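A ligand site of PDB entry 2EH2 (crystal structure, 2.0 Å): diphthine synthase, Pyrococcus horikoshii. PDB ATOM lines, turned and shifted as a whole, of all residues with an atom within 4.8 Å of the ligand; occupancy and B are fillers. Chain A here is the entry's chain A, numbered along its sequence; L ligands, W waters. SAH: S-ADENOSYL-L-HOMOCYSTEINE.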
ATOM      1  N   LEU A  10      -3.691 -20.113  19.109  1.00  0.00           N
ATOM      2  CA  LEU A  10      -3.213 -18.739  18.925  1.00  0.00           C
ATOM      3  C   LEU A  10      -3.921 -17.526  19.504  1.00  0.00           C
ATOM      4  O   LEU A  10      -3.250 -16.595  19.973  1.00  0.00           O
ATOM      5  CB  LEU A  10      -3.085 -18.476  17.425  1.00  0.00           C
ATOM      6  CG  LEU A  10      -2.196 -19.366  16.550  1.00  0.00           C
ATOM      7  CD1 LEU A  10      -2.625 -19.227  15.090  1.00  0.00           C
ATOM      8  CD2 LEU A  10      -0.742 -18.982  16.751  1.00  0.00           C
ATOM      9  N   TYR A  11      -5.240 -17.507  19.452  1.00  0.00           N
ATOM     10  CA  TYR A  11      -5.969 -16.311  19.869  1.00  0.00           C
ATOM     11  C   TYR A  11      -7.138 -16.477  20.843  1.00  0.00           C
ATOM     12  O   TYR A  11      -7.221 -15.754  21.834  1.00  0.00           O
ATOM     13  CB  TYR A  11      -6.450 -15.623  18.592  1.00  0.00           C
ATOM     14  CG  TYR A  11      -7.114 -14.275  18.773  1.00  0.00           C
ATOM     15  CD1 TYR A  11      -6.373 -13.147  19.144  1.00  0.00           C
ATOM     16  CD2 TYR A  11      -8.474 -14.119  18.523  1.00  0.00           C
ATOM     17  CE1 TYR A  11      -6.988 -11.899  19.269  1.00  0.00           C
ATOM     18  CE2 TYR A  11      -9.089 -12.877  18.641  1.00  0.00           C
ATOM     19  CZ  TYR A  11      -8.345 -11.778  19.010  1.00  0.00           C
ATOM     20  OH  TYR A  11      -8.960 -10.556  19.093  1.00  0.00           O
ATOM     21  N   THR A  36       3.700 -18.243  29.173  1.00  0.00           N
ATOM     22  CA  THR A  36       4.543 -18.436  27.988  1.00  0.00           C
ATOM     23  C   THR A  36       4.056 -17.671  26.763  1.00  0.00           C
ATOM     24  O   THR A  36       4.799 -17.477  25.816  1.00  0.00           O
ATOM     25  CB  THR A  36       4.683 -19.930  27.609  1.00  0.00           C
ATOM     26  OG1 THR A  36       3.387 -20.510  27.446  1.00  0.00           O
ATOM     27  CG2 THR A  36       5.451 -20.684  28.684  1.00  0.00           C
ATOM     28  N   SER A  37       2.804 -17.241  26.781  1.00  0.00           N
ATOM     29  CA  SER A  37       2.255 -16.488  25.660  1.00  0.00           C
ATOM     30  C   SER A  37       0.977 -15.776  26.057  1.00  0.00           C
ATOM     31  O   SER A  37       0.521 -15.892  27.189  1.00  0.00           O
ATOM     32  CB  SER A  37       1.985 -17.423  24.470  1.00  0.00           C
ATOM     33  OG  SER A  37       1.637 -16.680  23.312  1.00  0.00           O
ATOM     34  N   LEU A  38       0.396 -15.054  25.115  1.00  0.00           N
ATOM     35  CA  LEU A  38      -0.834 -14.324  25.374  1.00  0.00           C
ATOM     36  C   LEU A  38      -1.940 -14.659  24.373  1.00  0.00           C
ATOM     37  O   LEU A  38      -1.749 -14.564  23.169  1.00  0.00           O
ATOM     38  CB  LEU A  38      -0.576 -12.810  25.311  1.00  0.00           C
ATOM     39  CG  LEU A  38      -1.810 -11.910  25.383  1.00  0.00           C
ATOM     40  CD1 LEU A  38      -2.497 -12.069  26.738  1.00  0.00           C
ATOM     41  CD2 LEU A  38      -1.416 -10.452  25.158  1.00  0.00           C
ATOM     42  N   PRO A  85      -0.968 -21.880  26.033  1.00  0.00           N
ATOM     43  CA  PRO A  85      -1.353 -21.098  24.851  1.00  0.00           C
ATOM     44  C   PRO A  85      -0.610 -21.722  23.668  1.00  0.00           C
ATOM     45  O   PRO A  85       0.407 -22.402  23.874  1.00  0.00           O
ATOM     46  CB  PRO A  85      -0.830 -19.702  25.168  1.00  0.00           C
ATOM     47  CG  PRO A  85      -0.823 -19.657  26.673  1.00  0.00           C
ATOM     48  CD  PRO A  85      -0.308 -21.028  27.041  1.00  0.00           C
ATOM     49  N   GLY A  86      -1.101 -21.507  22.450  1.00  0.00           N
ATOM     50  CA  GLY A  86      -0.446 -22.063  21.269  1.00  0.00           C
ATOM     51  C   GLY A  86      -0.147 -23.544  21.403  1.00  0.00           C
ATOM     52  O   GLY A  86      -0.978 -24.301  21.901  1.00  0.00           O
ATOM     53  N   ASP A  87       1.030 -23.972  20.929  1.00  0.00           N
ATOM     54  CA  ASP A  87       1.447 -25.366  21.028  1.00  0.00           C
ATOM     55  C   ASP A  87       2.282 -25.458  22.308  1.00  0.00           C
ATOM     56  O   ASP A  87       3.203 -24.674  22.513  1.00  0.00           O
ATOM     57  CB  ASP A  87       2.273 -25.780  19.802  1.00  0.00           C
ATOM     58  CG  ASP A  87       2.694 -27.242  19.842  1.00  0.00           C
ATOM     59  OD1 ASP A  87       3.509 -27.599  20.712  1.00  0.00           O
ATOM     60  OD2 ASP A  87       2.209 -28.023  18.993  1.00  0.00           O
ATOM     61  N   VAL A  90       6.343 -25.526  21.810  1.00  0.00           N
ATOM     62  CA  VAL A  90       6.992 -24.591  20.919  1.00  0.00           C
ATOM     63  C   VAL A  90       7.391 -23.325  21.668  1.00  0.00           C
ATOM     64  O   VAL A  90       6.540 -22.626  22.215  1.00  0.00           O
ATOM     65  CB  VAL A  90       6.058 -24.201  19.740  1.00  0.00           C
ATOM     66  CG1 VAL A  90       6.704 -23.118  18.904  1.00  0.00           C
ATOM     67  CG2 VAL A  90       5.760 -25.437  18.899  1.00  0.00           C
ATOM     68  N   ALA A  91       8.690 -23.031  21.688  1.00  0.00           N
ATOM     69  CA  ALA A  91       9.194 -21.843  22.362  1.00  0.00           C
ATOM     70  C   ALA A  91       8.864 -21.858  23.856  1.00  0.00           C
ATOM     71  O   ALA A  91       8.502 -20.832  24.431  1.00  0.00           O
ATOM     72  CB  ALA A  91       8.650 -20.579  21.709  1.00  0.00           C
ATOM     73  N   THR A  92       8.970 -23.036  24.454  1.00  0.00           N
ATOM     74  CA  THR A  92       8.746 -23.215  25.886  1.00  0.00           C
ATOM     75  C   THR A  92       9.733 -24.310  26.260  1.00  0.00           C
ATOM     76  O   THR A  92      10.357 -24.917  25.386  1.00  0.00           O
ATOM     77  CB  THR A  92       7.339 -23.748  26.209  1.00  0.00           C
ATOM     78  OG1 THR A  92       7.260 -25.117  25.787  1.00  0.00           O
ATOM     79  CG2 THR A  92       6.258 -22.930  25.500  1.00  0.00           C
ATOM     80  N   PRO A 114      -2.617 -24.899  16.883  1.00  0.00           N
ATOM     81  CA  PRO A 114      -1.919 -23.937  16.025  1.00  0.00           C
ATOM     82  C   PRO A 114      -0.874 -23.146  16.816  1.00  0.00           C
ATOM     83  O   PRO A 114      -1.134 -22.712  17.934  1.00  0.00           O
ATOM     84  CB  PRO A 114      -3.055 -23.067  15.471  1.00  0.00           C
ATOM     85  CG  PRO A 114      -4.170 -23.255  16.455  1.00  0.00           C
ATOM     86  CD  PRO A 114      -4.070 -24.703  16.811  1.00  0.00           C
ATOM     87  N   SER A 115       0.306 -23.000  16.217  1.00  0.00           N
ATOM     88  CA  SER A 115       1.440 -22.305  16.828  1.00  0.00           C
ATOM     89  C   SER A 115       1.870 -21.099  16.005  1.00  0.00           C
ATOM     90  O   SER A 115       1.767 -21.101  14.771  1.00  0.00           O
ATOM     91  CB  SER A 115       2.616 -23.276  16.943  1.00  0.00           C
ATOM     92  OG  SER A 115       3.808 -22.609  17.336  1.00  0.00           O
ATOM     93  N   ILE A 116       2.372 -20.067  16.675  1.00  0.00           N
ATOM     94  CA  ILE A 116       2.822 -18.877  15.963  1.00  0.00           C
ATOM     95  C   ILE A 116       3.997 -19.232  15.038  1.00  0.00           C
ATOM     96  O   ILE A 116       4.197 -18.600  14.004  1.00  0.00           O
ATOM     97  CB  ILE A 116       3.257 -17.758  16.946  1.00  0.00           C
ATOM     98  CG1 ILE A 116       3.569 -16.467  16.177  1.00  0.00           C
ATOM     99  CG2 ILE A 116       4.471 -18.201  17.747  1.00  0.00           C
ATOM    100  CD1 ILE A 116       2.373 -15.889  15.429  1.00  0.00           C
ATOM    101  N   TYR A 117       4.754 -20.254  15.418  1.00  0.00           N
ATOM    102  CA  TYR A 117       5.910 -20.696  14.641  1.00  0.00           C
ATOM    103  C   TYR A 117       5.550 -21.047  13.191  1.00  0.00           C
ATOM    104  O   TYR A 117       6.313 -20.746  12.267  1.00  0.00           O
ATOM    105  CB  TYR A 117       6.562 -21.892  15.358  1.00  0.00           C
ATOM    106  CG  TYR A 117       7.826 -22.455  14.740  1.00  0.00           C
ATOM    107  CD1 TYR A 117       8.958 -21.660  14.545  1.00  0.00           C
ATOM    108  CD2 TYR A 117       7.888 -23.795  14.364  1.00  0.00           C
ATOM    109  CE1 TYR A 117      10.134 -22.207  14.005  1.00  0.00           C
ATOM    110  CE2 TYR A 117       9.055 -24.351  13.831  1.00  0.00           C
ATOM    111  CZ  TYR A 117      10.169 -23.551  13.660  1.00  0.00           C
ATOM    112  OH  TYR A 117      11.306 -24.110  13.115  1.00  0.00           O
ATOM    113  N   PHE A 165      10.607 -14.137  18.257  1.00  0.00           N
ATOM    114  CA  PHE A 165       9.584 -14.224  19.286  1.00  0.00           C
ATOM    115  C   PHE A 165       9.845 -12.993  20.158  1.00  0.00           C
ATOM    116  O   PHE A 165      10.997 -12.617  20.369  1.00  0.00           O
ATOM    117  CB  PHE A 165       9.778 -15.486  20.130  1.00  0.00           C
ATOM    118  CG  PHE A 165       9.512 -16.772  19.377  1.00  0.00           C
ATOM    119  CD1 PHE A 165       8.216 -17.285  19.316  1.00  0.00           C
ATOM    120  CD2 PHE A 165      10.539 -17.463  18.759  1.00  0.00           C
ATOM    121  CE1 PHE A 165       7.967 -18.494  18.642  1.00  0.00           C
ATOM    122  CE2 PHE A 165      10.299 -18.670  18.085  1.00  0.00           C
ATOM    123  CZ  PHE A 165       9.004 -19.183  18.037  1.00  0.00           C
ATOM    124  N   LEU A 166       8.787 -12.366  20.656  1.00  0.00           N
ATOM    125  CA  LEU A 166       8.950 -11.181  21.485  1.00  0.00           C
ATOM    126  C   LEU A 166       8.707 -11.527  22.949  1.00  0.00           C
ATOM    127  O   LEU A 166       7.908 -12.409  23.264  1.00  0.00           O
ATOM    128  CB  LEU A 166       8.013 -10.076  21.008  1.00  0.00           C
ATOM    129  CG  LEU A 166       8.213  -9.727  19.526  1.00  0.00           C
ATOM    130  CD1 LEU A 166       7.393  -8.499  19.170  1.00  0.00           C
ATOM    131  CD2 LEU A 166       9.689  -9.487  19.246  1.00  0.00           C
ATOM    132  N   ASP A 167       9.418 -10.835  23.835  1.00  0.00           N
ATOM    133  CA  ASP A 167       9.334 -11.083  25.268  1.00  0.00           C
ATOM    134  C   ASP A 167       7.957 -10.840  25.880  1.00  0.00           C
ATOM    135  O   ASP A 167       7.122 -10.120  25.327  1.00  0.00           O
ATOM    136  CB  ASP A 167      10.366 -10.227  25.998  1.00  0.00           C
ATOM    137  CG  ASP A 167      10.935 -10.911  27.233  1.00  0.00           C
ATOM    138  OD1 ASP A 167      10.470 -12.026  27.586  1.00  0.00           O
ATOM    139  OD2 ASP A 167      11.852 -10.335  27.851  1.00  0.00           O
ATOM    140  N   ILE A 168       7.734 -11.458  27.037  1.00  0.00           N
ATOM    141  CA  ILE A 168       6.489 -11.310  27.770  1.00  0.00           C
ATOM    142  C   ILE A 168       6.734 -11.486  29.271  1.00  0.00           C
ATOM    143  O   ILE A 168       7.394 -12.429  29.697  1.00  0.00           O
ATOM    144  CB  ILE A 168       5.416 -12.338  27.308  1.00  0.00           C
ATOM    145  CG1 ILE A 168       4.276 -12.388  28.326  1.00  0.00           C
ATOM    146  CG2 ILE A 168       6.041 -13.711  27.121  1.00  0.00           C
ATOM    147  CD1 ILE A 168       3.110 -13.272  27.917  1.00  0.00           C
ATOM    148  N   LEU A 206       3.558  -9.377  12.444  1.00  0.00           N
ATOM    149  CA  LEU A 206       2.321 -10.151  12.491  1.00  0.00           C
ATOM    150  C   LEU A 206       1.781  -9.981  13.901  1.00  0.00           C
ATOM    151  O   LEU A 206       2.451 -10.324  14.874  1.00  0.00           O
ATOM    152  CB  LEU A 206       2.589 -11.634  12.202  1.00  0.00           C
ATOM    153  CG  LEU A 206       1.388 -12.577  12.327  1.00  0.00           C
ATOM    154  CD1 LEU A 206       0.265 -12.112  11.428  1.00  0.00           C
ATOM    155  CD2 LEU A 206       1.805 -14.010  11.956  1.00  0.00           C
ATOM    156  N   ALA A 207       0.590  -9.413  14.010  1.00  0.00           N
ATOM    157  CA  ALA A 207      -0.026  -9.191  15.313  1.00  0.00           C
ATOM    158  C   ALA A 207      -1.366  -9.894  15.442  1.00  0.00           C
ATOM    159  O   ALA A 207      -2.209  -9.825  14.552  1.00  0.00           O
ATOM    160  CB  ALA A 207      -0.196  -7.696  15.567  1.00  0.00           C
ATOM    161  N   ARG A 208      -1.553 -10.571  16.573  1.00  0.00           N
ATOM    162  CA  ARG A 208      -2.787 -11.296  16.863  1.00  0.00           C
ATOM    163  C   ARG A 208      -3.123 -12.352  15.824  1.00  0.00           C
ATOM    164  O   ARG A 208      -4.244 -12.415  15.321  1.00  0.00           O
ATOM    165  CB  ARG A 208      -3.945 -10.305  17.017  1.00  0.00           C
ATOM    166  CG  ARG A 208      -3.716  -9.257  18.113  1.00  0.00           C
ATOM    167  CD  ARG A 208      -4.846  -8.237  18.145  1.00  0.00           C
ATOM    168  NE  ARG A 208      -5.066  -7.637  16.838  1.00  0.00           N
ATOM    169  CZ  ARG A 208      -4.223  -6.796  16.235  1.00  0.00           C
ATOM    170  NH1 ARG A 208      -3.100  -6.431  16.838  1.00  0.00           N
ATOM    171  NH2 ARG A 208      -4.500  -6.335  15.028  1.00  0.00           N
ATOM    172  N   ALA A 209      -2.140 -13.178  15.482  1.00  0.00           N
ATOM    173  CA  ALA A 209      -2.364 -14.260  14.540  1.00  0.00           C
ATOM    174  C   ALA A 209      -3.455 -15.130  15.163  1.00  0.00           C
ATOM    175  O   ALA A 209      -3.543 -15.229  16.387  1.00  0.00           O
ATOM    176  CB  ALA A 209      -1.089 -15.072  14.347  1.00  0.00           C
ATOM    177  N   PRO A 233      -0.591 -10.110  21.229  1.00  0.00           N
ATOM    178  CA  PRO A 233       0.845 -10.268  21.005  1.00  0.00           C
ATOM    179  C   PRO A 233       1.319  -9.975  19.585  1.00  0.00           C
ATOM    180  O   PRO A 233       0.548 -10.037  18.629  1.00  0.00           O
ATOM    181  CB  PRO A 233       1.080 -11.723  21.400  1.00  0.00           C
ATOM    182  CG  PRO A 233      -0.146 -12.374  20.854  1.00  0.00           C
ATOM    183  CD  PRO A 233      -1.260 -11.415  21.259  1.00  0.00           C
ATOM    184  N   HIS A 234       2.606  -9.663  19.464  1.00  0.00           N
ATOM    185  CA  HIS A 234       3.231  -9.364  18.182  1.00  0.00           C
ATOM    186  C   HIS A 234       4.454 -10.247  17.997  1.00  0.00           C
ATOM    187  O   HIS A 234       5.030 -10.742  18.960  1.00  0.00           O
ATOM    188  CB  HIS A 234       3.741  -7.921  18.139  1.00  0.00           C
ATOM    189  CG  HIS A 234       2.689  -6.868  18.322  1.00  0.00           C
ATOM    190  ND1 HIS A 234       2.987  -5.524  18.379  1.00  0.00           N
ATOM    191  CD2 HIS A 234       1.346  -6.959  18.439  1.00  0.00           C
ATOM    192  CE1 HIS A 234       1.875  -4.834  18.528  1.00  0.00           C
ATOM    193  NE2 HIS A 234       0.859  -5.681  18.570  1.00  0.00           N
ATOM    194  N   ILE A 235       4.837 -10.441  16.741  1.00  0.00           N
ATOM    195  CA  ILE A 235       6.032 -11.179  16.407  1.00  0.00           C
ATOM    196  C   ILE A 235       6.700 -10.342  15.349  1.00  0.00           C
ATOM    197  O   ILE A 235       6.017  -9.680  14.569  1.00  0.00           O
ATOM    198  CB  ILE A 235       5.761 -12.571  15.822  1.00  0.00           C
ATOM    199  CG1 ILE A 235       4.754 -12.469  14.677  1.00  0.00           C
ATOM    200  CG2 ILE A 235       5.296 -13.498  16.890  1.00  0.00           C
ATOM    201  CD1 ILE A 235       4.505 -13.769  13.993  1.00  0.00           C
HETATM  202  N   SAH L   1       3.969 -22.088  22.454  1.00  0.00           N
HETATM  203  CA  SAH L   1       3.607 -20.766  21.767  1.00  0.00           C
HETATM  204  CB  SAH L   1       4.688 -19.718  21.704  1.00  0.00           C
HETATM  205  CG  SAH L   1       5.304 -19.224  23.017  1.00  0.00           C
HETATM  206  SD  SAH L   1       6.374 -17.774  22.647  1.00  0.00           S
HETATM  207  C   SAH L   1       3.108 -21.141  20.306  1.00  0.00           C
HETATM  208  O   SAH L   1       3.094 -22.341  19.961  1.00  0.00           O
HETATM  209  OXT SAH L   1       2.731 -20.167  19.546  1.00  0.00           O
HETATM  210  C5' SAH L   1       5.206 -16.487  22.867  1.00  0.00           C
HETATM  211  C4' SAH L   1       5.546 -15.300  21.894  1.00  0.00           C
HETATM  212  O4' SAH L   1       5.225 -15.744  20.544  1.00  0.00           O
HETATM  213  C3' SAH L   1       4.777 -14.045  22.131  1.00  0.00           C
HETATM  214  O3' SAH L   1       5.463 -13.208  23.058  1.00  0.00           O
HETATM  215  C2' SAH L   1       4.661 -13.478  20.694  1.00  0.00           C
HETATM  216  O2' SAH L   1       5.839 -12.743  20.338  1.00  0.00           O
HETATM  217  C1' SAH L   1       4.421 -14.721  19.820  1.00  0.00           C
HETATM  218  N9  SAH L   1       3.116 -15.105  19.706  1.00  0.00           N
HETATM  219  C8  SAH L   1       2.338 -16.100  20.265  1.00  0.00           C
HETATM  220  N7  SAH L   1       1.099 -16.131  19.864  1.00  0.00           N
HETATM  221  C5  SAH L   1       1.002 -15.061  18.930  1.00  0.00           C
HETATM  222  C6  SAH L   1      -0.106 -14.584  18.129  1.00  0.00           C
HETATM  223  N6  SAH L   1      -1.331 -15.127  18.153  1.00  0.00           N
HETATM  224  N1  SAH L   1       0.180 -13.509  17.327  1.00  0.00           N
HETATM  225  C2  SAH L   1       1.418 -12.927  17.267  1.00  0.00           C
HETATM  226  N3  SAH L   1       2.495 -13.355  18.008  1.00  0.00           N
HETATM  227  C4  SAH L   1       2.219 -14.422  18.816  1.00  0.00           C
HETATM  228  O   HOH W   1       2.891 -21.296  24.959  1.00  0.00           O
HETATM  229  O   HOH W   2       0.111 -18.762  20.245  1.00  0.00           O
HETATM  230  O   HOH W   3       4.713 -10.657  24.139  1.00  0.00           O
HETATM  231  O   HOH W   4      -0.798 -17.371  22.335  1.00  0.00           O
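Water W1 lies within hydrogen-bond range of OG1 of Thr 36, N of the ligand and O of Pro 85.
Water W3 lies within hydrogen-bond range of the backbone carbonyl oxygen of Asp 167 (2.7 Å) and an oxygen (O3') of the ligand (2.9 Å).
The backbone carbonyl oxygen (O) of Pro 233 lies within hydrogen-bond range of the backbone NH (N) of Arg 208 (3.0 Å).
OG of Ser 115 lies close to N of Tyr 117.
The backbone NH of Ile 235 is in hydrogen-bond range of the backbone carbonyl oxygen of Leu 206, at 3.0 Å.
A nitrogen (N) of the ligand lies within hydrogen-bond range of the backbone carbonyl oxygen (O) of Asp 87.
A nitrogen (N6) of the ligand is in hydrogen-bond range of the backbone carbonyl oxygen of Leu 10 (3.0 Å).
The backbone NH of Leu 166 sits at hydrogen-bond distance from an oxygen (O2') of the ligand (3.0 Å).
N of Ile 116 lies within hydrogen-bond range of OXT of the ligand.
O of Leu 166 is in hydrogen-bond range of O3' of the ligand (2.6 Å).
O of Val 90 is in hydrogen-bond range of N of the ligand, at 2.6 Å.
The backbone carbonyl oxygen (O) of His 234 is in hydrogen-bond range of an oxygen (O2') of the ligand, 2.6 Å away.
N1 of the ligand sits at hydrogen-bond distance from N of Ala 209 (3.0 Å).
OG of Ser 115 lies within hydrogen-bond range of O of the ligand (2.7 Å).
The backbone NH (N) of Arg 208 lies within hydrogen-bond range of a nitrogen (N1) of the ligand, 3.5 Å away.
An oxygen (O) of the ligand lies within hydrogen-bond range of the backbone NH (N) of Asp 87, 2.8 Å away.
The backbone carbonyl oxygen (O) of Ala 209 sits at hydrogen-bond distance from a nitrogen (N6) of the ligand (2.8 Å).
O of Thr 36 sits close to SD of the ligand, 3.6 Å away.
Residues that only touch the ligand: Ser 37 (3.2 Å), Pro 85 (3.8 Å), Gly 86 (3.7 Å), Ala 91 (3.7 Å), Thr 92 (3.9 Å), Phe 165 (3.6 Å), Leu 206 (3.7 Å), Pro 233 (3.3 Å) and Ile 235 (3.0 Å).
Hydrophobic or aromatic side chains that line the ligand: Leu 10, Val 90, Ala 91, Ile 116, Phe 165, Leu 166, Ala 209, Pro 233 and Ile 235.
19 residues have an atom within 4 Å of the ligand: Leu 10, Thr 36, Ser 37, Pro 85, Gly 86, Asp 87, Val 90, Ala 91, Thr 92, Ser 115, Ile 116, Phe 165, Leu 166, Leu 206, Arg 208, Ala 209, Pro 233, His 234 and Ile 235.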
